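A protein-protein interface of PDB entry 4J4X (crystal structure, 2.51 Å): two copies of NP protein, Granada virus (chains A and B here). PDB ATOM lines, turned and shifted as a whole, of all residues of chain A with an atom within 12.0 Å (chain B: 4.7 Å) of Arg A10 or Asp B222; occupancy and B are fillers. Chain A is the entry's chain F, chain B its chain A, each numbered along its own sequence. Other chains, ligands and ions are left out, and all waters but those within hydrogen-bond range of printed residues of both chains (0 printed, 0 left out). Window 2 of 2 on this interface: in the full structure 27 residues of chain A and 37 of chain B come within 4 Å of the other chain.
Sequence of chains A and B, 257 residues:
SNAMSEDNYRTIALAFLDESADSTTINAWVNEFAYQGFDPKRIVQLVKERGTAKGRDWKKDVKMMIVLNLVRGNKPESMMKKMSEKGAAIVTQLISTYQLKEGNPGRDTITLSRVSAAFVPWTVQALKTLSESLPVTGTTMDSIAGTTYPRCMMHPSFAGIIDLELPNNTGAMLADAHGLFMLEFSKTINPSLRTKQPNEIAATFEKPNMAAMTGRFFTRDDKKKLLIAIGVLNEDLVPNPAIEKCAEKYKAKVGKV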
ATOM      1  N   ASN A   8       9.389 -22.883  26.857  1.00  0.00           N
ATOM      2  CA  ASN A   8      10.362 -22.056  26.186  1.00  0.00           C
ATOM      3  C   ASN A   8      11.595 -21.785  27.003  1.00  0.00           C
ATOM      4  O   ASN A   8      11.554 -21.109  27.980  1.00  0.00           O
ATOM      5  CB  ASN A   8       9.732 -20.750  25.762  1.00  0.00           C
ATOM      6  CG  ASN A   8      10.708 -19.833  25.075  1.00  0.00           C
ATOM      7  OD1 ASN A   8      11.752 -20.248  24.599  1.00  0.00           O
ATOM      8  ND2 ASN A   8      10.363 -18.573  25.026  1.00  0.00           N
ATOM      9  N   TYR A   9      12.689 -22.353  26.561  1.00  0.00           N
ATOM     10  CA  TYR A   9      13.944 -22.329  27.263  1.00  0.00           C
ATOM     11  C   TYR A   9      14.606 -20.992  27.450  1.00  0.00           C
ATOM     12  O   TYR A   9      15.219 -20.765  28.446  1.00  0.00           O
ATOM     13  CB  TYR A   9      14.873 -23.355  26.670  1.00  0.00           C
ATOM     14  CG  TYR A   9      14.233 -24.683  26.727  1.00  0.00           C
ATOM     15  CD1 TYR A   9      13.738 -25.145  27.898  1.00  0.00           C
ATOM     16  CD2 TYR A   9      14.064 -25.445  25.616  1.00  0.00           C
ATOM     17  CE1 TYR A   9      13.114 -26.351  27.978  1.00  0.00           C
ATOM     18  CE2 TYR A   9      13.453 -26.663  25.686  1.00  0.00           C
ATOM     19  CZ  TYR A   9      12.974 -27.106  26.878  1.00  0.00           C
ATOM     20  OH  TYR A   9      12.349 -28.307  26.992  1.00  0.00           O
ATOM     21  N   ARG A  10      14.509 -20.128  26.468  1.00  0.00           N
ATOM     22  CA  ARG A  10      15.119 -18.843  26.569  1.00  0.00           C
ATOM     23  C   ARG A  10      14.454 -18.098  27.685  1.00  0.00           C
ATOM     24  O   ARG A  10      15.076 -17.433  28.473  1.00  0.00           O
ATOM     25  CB  ARG A  10      14.959 -18.111  25.238  1.00  0.00           C
ATOM     26  CG  ARG A  10      15.127 -16.609  25.279  1.00  0.00           C
ATOM     27  CD  ARG A  10      14.920 -15.979  23.925  1.00  0.00           C
ATOM     28  NE  ARG A  10      13.520 -15.932  23.605  1.00  0.00           N
ATOM     29  CZ  ARG A  10      12.669 -15.072  24.129  1.00  0.00           C
ATOM     30  NH1 ARG A  10      13.074 -14.170  24.983  1.00  0.00           N
ATOM     31  NH2 ARG A  10      11.411 -15.118  23.790  1.00  0.00           N
ATOM     32  N   THR A  11      13.150 -18.209  27.693  1.00  0.00           N
ATOM     33  CA  THR A  11      12.274 -17.586  28.646  1.00  0.00           C
ATOM     34  C   THR A  11      12.405 -18.100  30.078  1.00  0.00           C
ATOM     35  O   THR A  11      12.278 -17.359  30.999  1.00  0.00           O
ATOM     36  CB  THR A  11      10.864 -17.494  28.043  1.00  0.00           C
ATOM     37  OG1 THR A  11      10.614 -16.136  27.715  1.00  0.00           O
ATOM     38  CG2 THR A  11       9.795 -17.992  28.935  1.00  0.00           C
ATOM     39  N   ILE A  12      12.638 -19.384  30.233  1.00  0.00           N
ATOM     40  CA  ILE A  12      12.893 -19.974  31.506  1.00  0.00           C
ATOM     41  C   ILE A  12      14.168 -19.420  32.089  1.00  0.00           C
ATOM     42  O   ILE A  12      14.241 -19.145  33.241  1.00  0.00           O
ATOM     43  CB  ILE A  12      12.975 -21.508  31.349  1.00  0.00           C
ATOM     44  CG1 ILE A  12      11.592 -22.093  31.284  1.00  0.00           C
ATOM     45  CG2 ILE A  12      13.695 -22.198  32.494  1.00  0.00           C
ATOM     46  CD1 ILE A  12      11.556 -23.511  30.808  1.00  0.00           C
ATOM     47  N   ALA A  13      15.190 -19.303  31.282  1.00  0.00           N
ATOM     48  CA  ALA A  13      16.441 -18.762  31.719  1.00  0.00           C
ATOM     49  C   ALA A  13      16.347 -17.313  32.124  1.00  0.00           C
ATOM     50  O   ALA A  13      16.958 -16.910  33.059  1.00  0.00           O
ATOM     51  CB  ALA A  13      17.495 -18.969  30.666  1.00  0.00           C
ATOM     52  N   LEU A  14      15.573 -16.532  31.408  1.00  0.00           N
ATOM     53  CA  LEU A  14      15.411 -15.135  31.711  1.00  0.00           C
ATOM     54  C   LEU A  14      14.706 -14.948  33.019  1.00  0.00           C
ATOM     55  O   LEU A  14      14.886 -13.972  33.680  1.00  0.00           O
ATOM     56  CB  LEU A  14      14.698 -14.406  30.590  1.00  0.00           C
ATOM     57  CG  LEU A  14      15.458 -14.326  29.279  1.00  0.00           C
ATOM     58  CD1 LEU A  14      14.559 -13.869  28.173  1.00  0.00           C
ATOM     59  CD2 LEU A  14      16.652 -13.423  29.355  1.00  0.00           C
ATOM     60  N   ALA A  15      13.921 -15.930  33.394  1.00  0.00           N
ATOM     61  CA  ALA A  15      13.142 -15.857  34.598  1.00  0.00           C
ATOM     62  C   ALA A  15      13.976 -15.807  35.858  1.00  0.00           C
ATOM     63  O   ALA A  15      13.514 -15.396  36.882  1.00  0.00           O
ATOM     64  CB  ALA A  15      12.137 -16.969  34.653  1.00  0.00           C
ATOM     65  N   PHE A  16      15.213 -16.230  35.766  1.00  0.00           N
ATOM     66  CA  PHE A  16      16.094 -16.249  36.902  1.00  0.00           C
ATOM     67  C   PHE A  16      16.556 -14.895  37.302  1.00  0.00           C
ATOM     68  O   PHE A  16      17.077 -14.725  38.343  1.00  0.00           O
ATOM     69  CB  PHE A  16      17.260 -17.179  36.687  1.00  0.00           C
ATOM     70  CG  PHE A  16      16.931 -18.607  36.912  1.00  0.00           C
ATOM     71  CD1 PHE A  16      16.095 -19.257  36.070  1.00  0.00           C
ATOM     72  CD2 PHE A  16      17.472 -19.296  37.959  1.00  0.00           C
ATOM     73  CE1 PHE A  16      15.800 -20.569  36.263  1.00  0.00           C
ATOM     74  CE2 PHE A  16      17.172 -20.609  38.161  1.00  0.00           C
ATOM     75  CZ  PHE A  16      16.337 -21.244  37.312  1.00  0.00           C
ATOM     76  N   LEU A  17      16.305 -13.928  36.468  1.00  0.00           N
ATOM     77  CA  LEU A  17      16.609 -12.560  36.774  1.00  0.00           C
ATOM     78  C   LEU A  17      15.824 -12.164  37.982  1.00  0.00           C
ATOM     79  O   LEU A  17      16.272 -11.387  38.770  1.00  0.00           O
ATOM     80  CB  LEU A  17      16.244 -11.654  35.618  1.00  0.00           C
ATOM     81  CG  LEU A  17      16.768 -10.250  35.819  1.00  0.00           C
ATOM     82  CD1 LEU A  17      18.264 -10.257  35.706  1.00  0.00           C
ATOM     83  CD2 LEU A  17      16.168  -9.277  34.847  1.00  0.00           C
ATOM     84  N   ASP A  18      14.631 -12.689  38.115  1.00  0.00           N
ATOM     85  CA  ASP A  18      13.840 -12.415  39.280  1.00  0.00           C
ATOM     86  C   ASP A  18      13.796 -13.527  40.302  1.00  0.00           C
ATOM     87  O   ASP A  18      13.022 -13.457  41.213  1.00  0.00           O
ATOM     88  CB  ASP A  18      12.426 -12.033  38.888  1.00  0.00           C
ATOM     89  CG  ASP A  18      12.379 -10.852  37.969  1.00  0.00           C
ATOM     90  OD1 ASP A  18      12.973  -9.816  38.290  1.00  0.00           O
ATOM     91  OD2 ASP A  18      11.739 -10.954  36.921  1.00  0.00           O
ATOM     92  N   GLU A  19      14.598 -14.561  40.140  1.00  0.00           N
ATOM     93  CA  GLU A  19      14.724 -15.567  41.169  1.00  0.00           C
ATOM     94  C   GLU A  19      15.502 -14.978  42.301  1.00  0.00           C
ATOM     95  O   GLU A  19      16.333 -14.148  42.083  1.00  0.00           O
ATOM     96  CB  GLU A  19      15.433 -16.803  40.659  1.00  0.00           C
ATOM     97  CG  GLU A  19      14.552 -17.783  39.926  1.00  0.00           C
ATOM     98  CD  GLU A  19      13.597 -18.520  40.823  1.00  0.00           C
ATOM     99  OE1 GLU A  19      13.898 -18.788  41.985  1.00  0.00           O
ATOM    100  OE2 GLU A  19      12.515 -18.833  40.355  1.00  0.00           O
ATOM    101  N   PHE B 217      21.058 -17.284  21.617  1.00  0.00           N
ATOM    102  CA  PHE B 217      20.174 -17.752  22.661  1.00  0.00           C
ATOM    103  C   PHE B 217      19.383 -16.645  23.300  1.00  0.00           C
ATOM    104  O   PHE B 217      18.214 -16.757  23.479  1.00  0.00           O
ATOM    105  CB  PHE B 217      20.970 -18.505  23.701  1.00  0.00           C
ATOM    106  CG  PHE B 217      20.157 -19.054  24.811  1.00  0.00           C
ATOM    107  CD1 PHE B 217      19.262 -20.061  24.604  1.00  0.00           C
ATOM    108  CD2 PHE B 217      20.318 -18.580  26.071  1.00  0.00           C
ATOM    109  CE1 PHE B 217      18.533 -20.572  25.638  1.00  0.00           C
ATOM    110  CE2 PHE B 217      19.602 -19.088  27.105  1.00  0.00           C
ATOM    111  CZ  PHE B 217      18.709 -20.083  26.890  1.00  0.00           C
ATOM    112  N   PHE B 218      20.039 -15.564  23.612  1.00  0.00           N
ATOM    113  CA  PHE B 218      19.354 -14.419  24.113  1.00  0.00           C
ATOM    114  C   PHE B 218      19.235 -13.416  22.998  1.00  0.00           C
ATOM    115  O   PHE B 218      20.076 -13.307  22.146  1.00  0.00           O
ATOM    116  CB  PHE B 218      20.093 -13.834  25.295  1.00  0.00           C
ATOM    117  CG  PHE B 218      19.970 -14.637  26.539  1.00  0.00           C
ATOM    118  CD1 PHE B 218      18.758 -14.922  27.060  1.00  0.00           C
ATOM    119  CD2 PHE B 218      21.080 -15.102  27.194  1.00  0.00           C
ATOM    120  CE1 PHE B 218      18.648 -15.661  28.203  1.00  0.00           C
ATOM    121  CE2 PHE B 218      20.977 -15.844  28.341  1.00  0.00           C
ATOM    122  CZ  PHE B 218      19.757 -16.119  28.844  1.00  0.00           C
ATOM    123  N   THR B 219      18.145 -12.713  22.989  1.00  0.00           N
ATOM    124  CA  THR B 219      17.849 -11.752  21.969  1.00  0.00           C
ATOM    125  C   THR B 219      18.507 -10.419  22.273  1.00  0.00           C
ATOM    126  O   THR B 219      18.875 -10.178  23.373  1.00  0.00           O
ATOM    127  CB  THR B 219      16.324 -11.728  21.829  1.00  0.00           C
ATOM    128  OG1 THR B 219      15.964 -12.589  20.767  1.00  0.00           O
ATOM    129  CG2 THR B 219      15.749 -10.399  21.580  1.00  0.00           C
ATOM    130  N   ARG B 220      18.615  -9.554  21.284  1.00  0.00           N
ATOM    131  CA  ARG B 220      19.223  -8.249  21.465  1.00  0.00           C
ATOM    132  C   ARG B 220      18.444  -7.436  22.456  1.00  0.00           C
ATOM    133  O   ARG B 220      18.973  -6.733  23.282  1.00  0.00           O
ATOM    134  CB  ARG B 220      19.219  -7.499  20.144  1.00  0.00           C
ATOM    135  CG  ARG B 220      20.315  -7.900  19.191  1.00  0.00           C
ATOM    136  CD  ARG B 220      20.863  -6.749  18.374  1.00  0.00           C
ATOM    137  NE  ARG B 220      19.951  -5.616  18.314  1.00  0.00           N
ATOM    138  CZ  ARG B 220      20.315  -4.343  18.377  1.00  0.00           C
ATOM    139  NH1 ARG B 220      21.574  -4.013  18.502  1.00  0.00           N
ATOM    140  NH2 ARG B 220      19.404  -3.399  18.322  1.00  0.00           N
ATOM    141  N   ASP B 221      17.151  -7.507  22.308  1.00  0.00           N
ATOM    142  CA  ASP B 221      16.252  -6.834  23.174  1.00  0.00           C
ATOM    143  C   ASP B 221      16.348  -7.389  24.585  1.00  0.00           C
ATOM    144  O   ASP B 221      16.235  -6.662  25.531  1.00  0.00           O
ATOM    145  CB  ASP B 221      14.866  -6.894  22.569  1.00  0.00           C
ATOM    146  CG  ASP B 221      13.806  -6.619  23.545  1.00  0.00           C
ATOM    147  OD1 ASP B 221      13.620  -5.449  23.923  1.00  0.00           O
ATOM    148  OD2 ASP B 221      13.159  -7.595  23.938  1.00  0.00           O
ATOM    149  N   ASP B 222      16.557  -8.689  24.705  1.00  0.00           N
ATOM    150  CA  ASP B 222      16.742  -9.318  25.994  1.00  0.00           C
ATOM    151  C   ASP B 222      17.959  -8.813  26.677  1.00  0.00           C
ATOM    152  O   ASP B 222      17.936  -8.554  27.844  1.00  0.00           O
ATOM    153  CB  ASP B 222      16.950 -10.807  25.828  1.00  0.00           C
ATOM    154  CG  ASP B 222      15.703 -11.533  25.533  1.00  0.00           C
ATOM    155  OD1 ASP B 222      14.708 -11.253  26.191  1.00  0.00           O
ATOM    156  OD2 ASP B 222      15.707 -12.396  24.655  1.00  0.00           O
ATOM    157  N   LYS B 223      19.042  -8.713  25.937  1.00  0.00           N
ATOM    158  CA  LYS B 223      20.298  -8.263  26.476  1.00  0.00           C
ATOM    159  C   LYS B 223      20.204  -6.854  26.980  1.00  0.00           C
ATOM    160  O   LYS B 223      20.776  -6.544  27.968  1.00  0.00           O
ATOM    161  CB  LYS B 223      21.393  -8.367  25.444  1.00  0.00           C
ATOM    162  CG  LYS B 223      21.937  -9.750  25.261  1.00  0.00           C
ATOM    163  CD  LYS B 223      22.585  -9.883  23.916  1.00  0.00           C
ATOM    164  CE  LYS B 223      23.283 -11.191  23.765  1.00  0.00           C
ATOM    165  NZ  LYS B 223      24.347 -11.122  22.769  1.00  0.00           N
ATOM    166  N   LYS B 224      19.465  -6.011  26.291  1.00  0.00           N
ATOM    167  CA  LYS B 224      19.246  -4.656  26.723  1.00  0.00           C
ATOM    168  C   LYS B 224      18.525  -4.643  28.026  1.00  0.00           C
ATOM    169  O   LYS B 224      18.828  -3.860  28.882  1.00  0.00           O
ATOM    170  CB  LYS B 224      18.381  -3.907  25.720  1.00  0.00           C
ATOM    171  CG  LYS B 224      19.115  -3.311  24.549  1.00  0.00           C
ATOM    172  CD  LYS B 224      18.148  -2.786  23.506  1.00  0.00           C
ATOM    173  CE  LYS B 224      18.854  -2.281  22.257  1.00  0.00           C
ATOM    174  NZ  LYS B 224      18.805  -3.239  21.125  1.00  0.00           N
ATOM    175  N   LYS B 225      17.538  -5.495  28.158  1.00  0.00           N
ATOM    176  CA  LYS B 225      16.783  -5.514  29.366  1.00  0.00           C
ATOM    177  C   LYS B 225      17.638  -5.896  30.571  1.00  0.00           C
ATOM    178  O   LYS B 225      17.524  -5.306  31.614  1.00  0.00           O
ATOM    179  CB  LYS B 225      15.550  -6.402  29.191  1.00  0.00           C
ATOM    180  CG  LYS B 225      15.088  -7.153  30.431  1.00  0.00           C
ATOM    181  CD  LYS B 225      13.621  -6.949  30.748  1.00  0.00           C
ATOM    182  CE  LYS B 225      13.220  -7.705  31.998  1.00  0.00           C
ATOM    183  NZ  LYS B 225      13.218  -6.830  33.190  1.00  0.00           N
ATOM    184  N   LEU B 226      18.484  -6.887  30.422  1.00  0.00           N
ATOM    185  CA  LEU B 226      19.353  -7.272  31.500  1.00  0.00           C
ATOM    186  C   LEU B 226      20.362  -6.240  31.905  1.00  0.00           C
ATOM    187  O   LEU B 226      20.618  -6.048  33.054  1.00  0.00           O
ATOM    188  CB  LEU B 226      20.096  -8.522  31.116  1.00  0.00           C
ATOM    189  CG  LEU B 226      19.194  -9.682  30.852  1.00  0.00           C
ATOM    190  CD1 LEU B 226      19.898 -10.661  29.962  1.00  0.00           C
ATOM    191  CD2 LEU B 226      18.849 -10.299  32.170  1.00  0.00           C
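Of the 12 printed residues of chain A, 4 touch a printed residue of chain B. Hydrophobic or aromatic side chains of chain A that line the printed part of chain B: Leu A14 and Leu A17. Among the printed residues, 7 pairs touch across the chains. Among the printed residues, Asp or Glu carboxylates within 4 Å of a Lys or Arg side-chain nitrogen of the other chain: Arg A10 with Asp B222 (3.2 Å).
Tyr A9 touches Phe B217. Arg A10 touches Phe B217 (CD to O, 3.4 Å). Phe B218 touches Arg A10 (CE1 to O, 3.997 Å). CD2 of Leu A14 touches CE1 of Phe B218, 3.2 Å away. CD1 of Leu A14 touches OD1 of Asp B222, at 3.3 Å. Leu B226 touches Leu A17 (CD2 to CD1, 3.6 Å).
The backbone NH of Thr B219 lies close to the side-chain carboxylate of Asp B222, 3.0 Å away. OD1 of Asn A8 lies within hydrogen-bond range of N of Arg A10, 3.3 Å away.
OD2 of Asp B222 is in salt-bridge range of NH1 of Arg A10, 3.2 Å away.
No position is printed for both chains. Of the 7 pairs that touch across the chains among the printed residues, none has its exchanged pair printed and touching as well.
Of the printed residues of chain B, Arg A10 touches Phe B217, Phe B218 and Asp B222. No residue of chain A comes within 4 Å of Thr B219. No residue of chain A comes within 4 Å of Asp B221. No residue of chain A comes within 4 Å of Lys B223. Lys B225 touches none of the printed residues of chain A. Leu B226 touches just one residue of chain A: Leu A17. Printed residues of chain B within 4 Å of Leu A17: Leu B226 (3.6 Å). Printed residues of chain B within 4 Å of Leu A14: Phe B218 and Asp B222. Of the printed residues of chain A, Phe B218 touches Arg A10 and Leu A14. Of the printed residues of chain B, Tyr A9 touches Phe B217 (3.9 Å). Ala A13 touches none of the printed residues of chain B. The nearest printed residue of chain B that does not touch Arg A10 is Thr B219 (4.7 Å). The nearest printed residue of chain A that does not touch Phe B218 is Ala A13 (4.1 Å).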
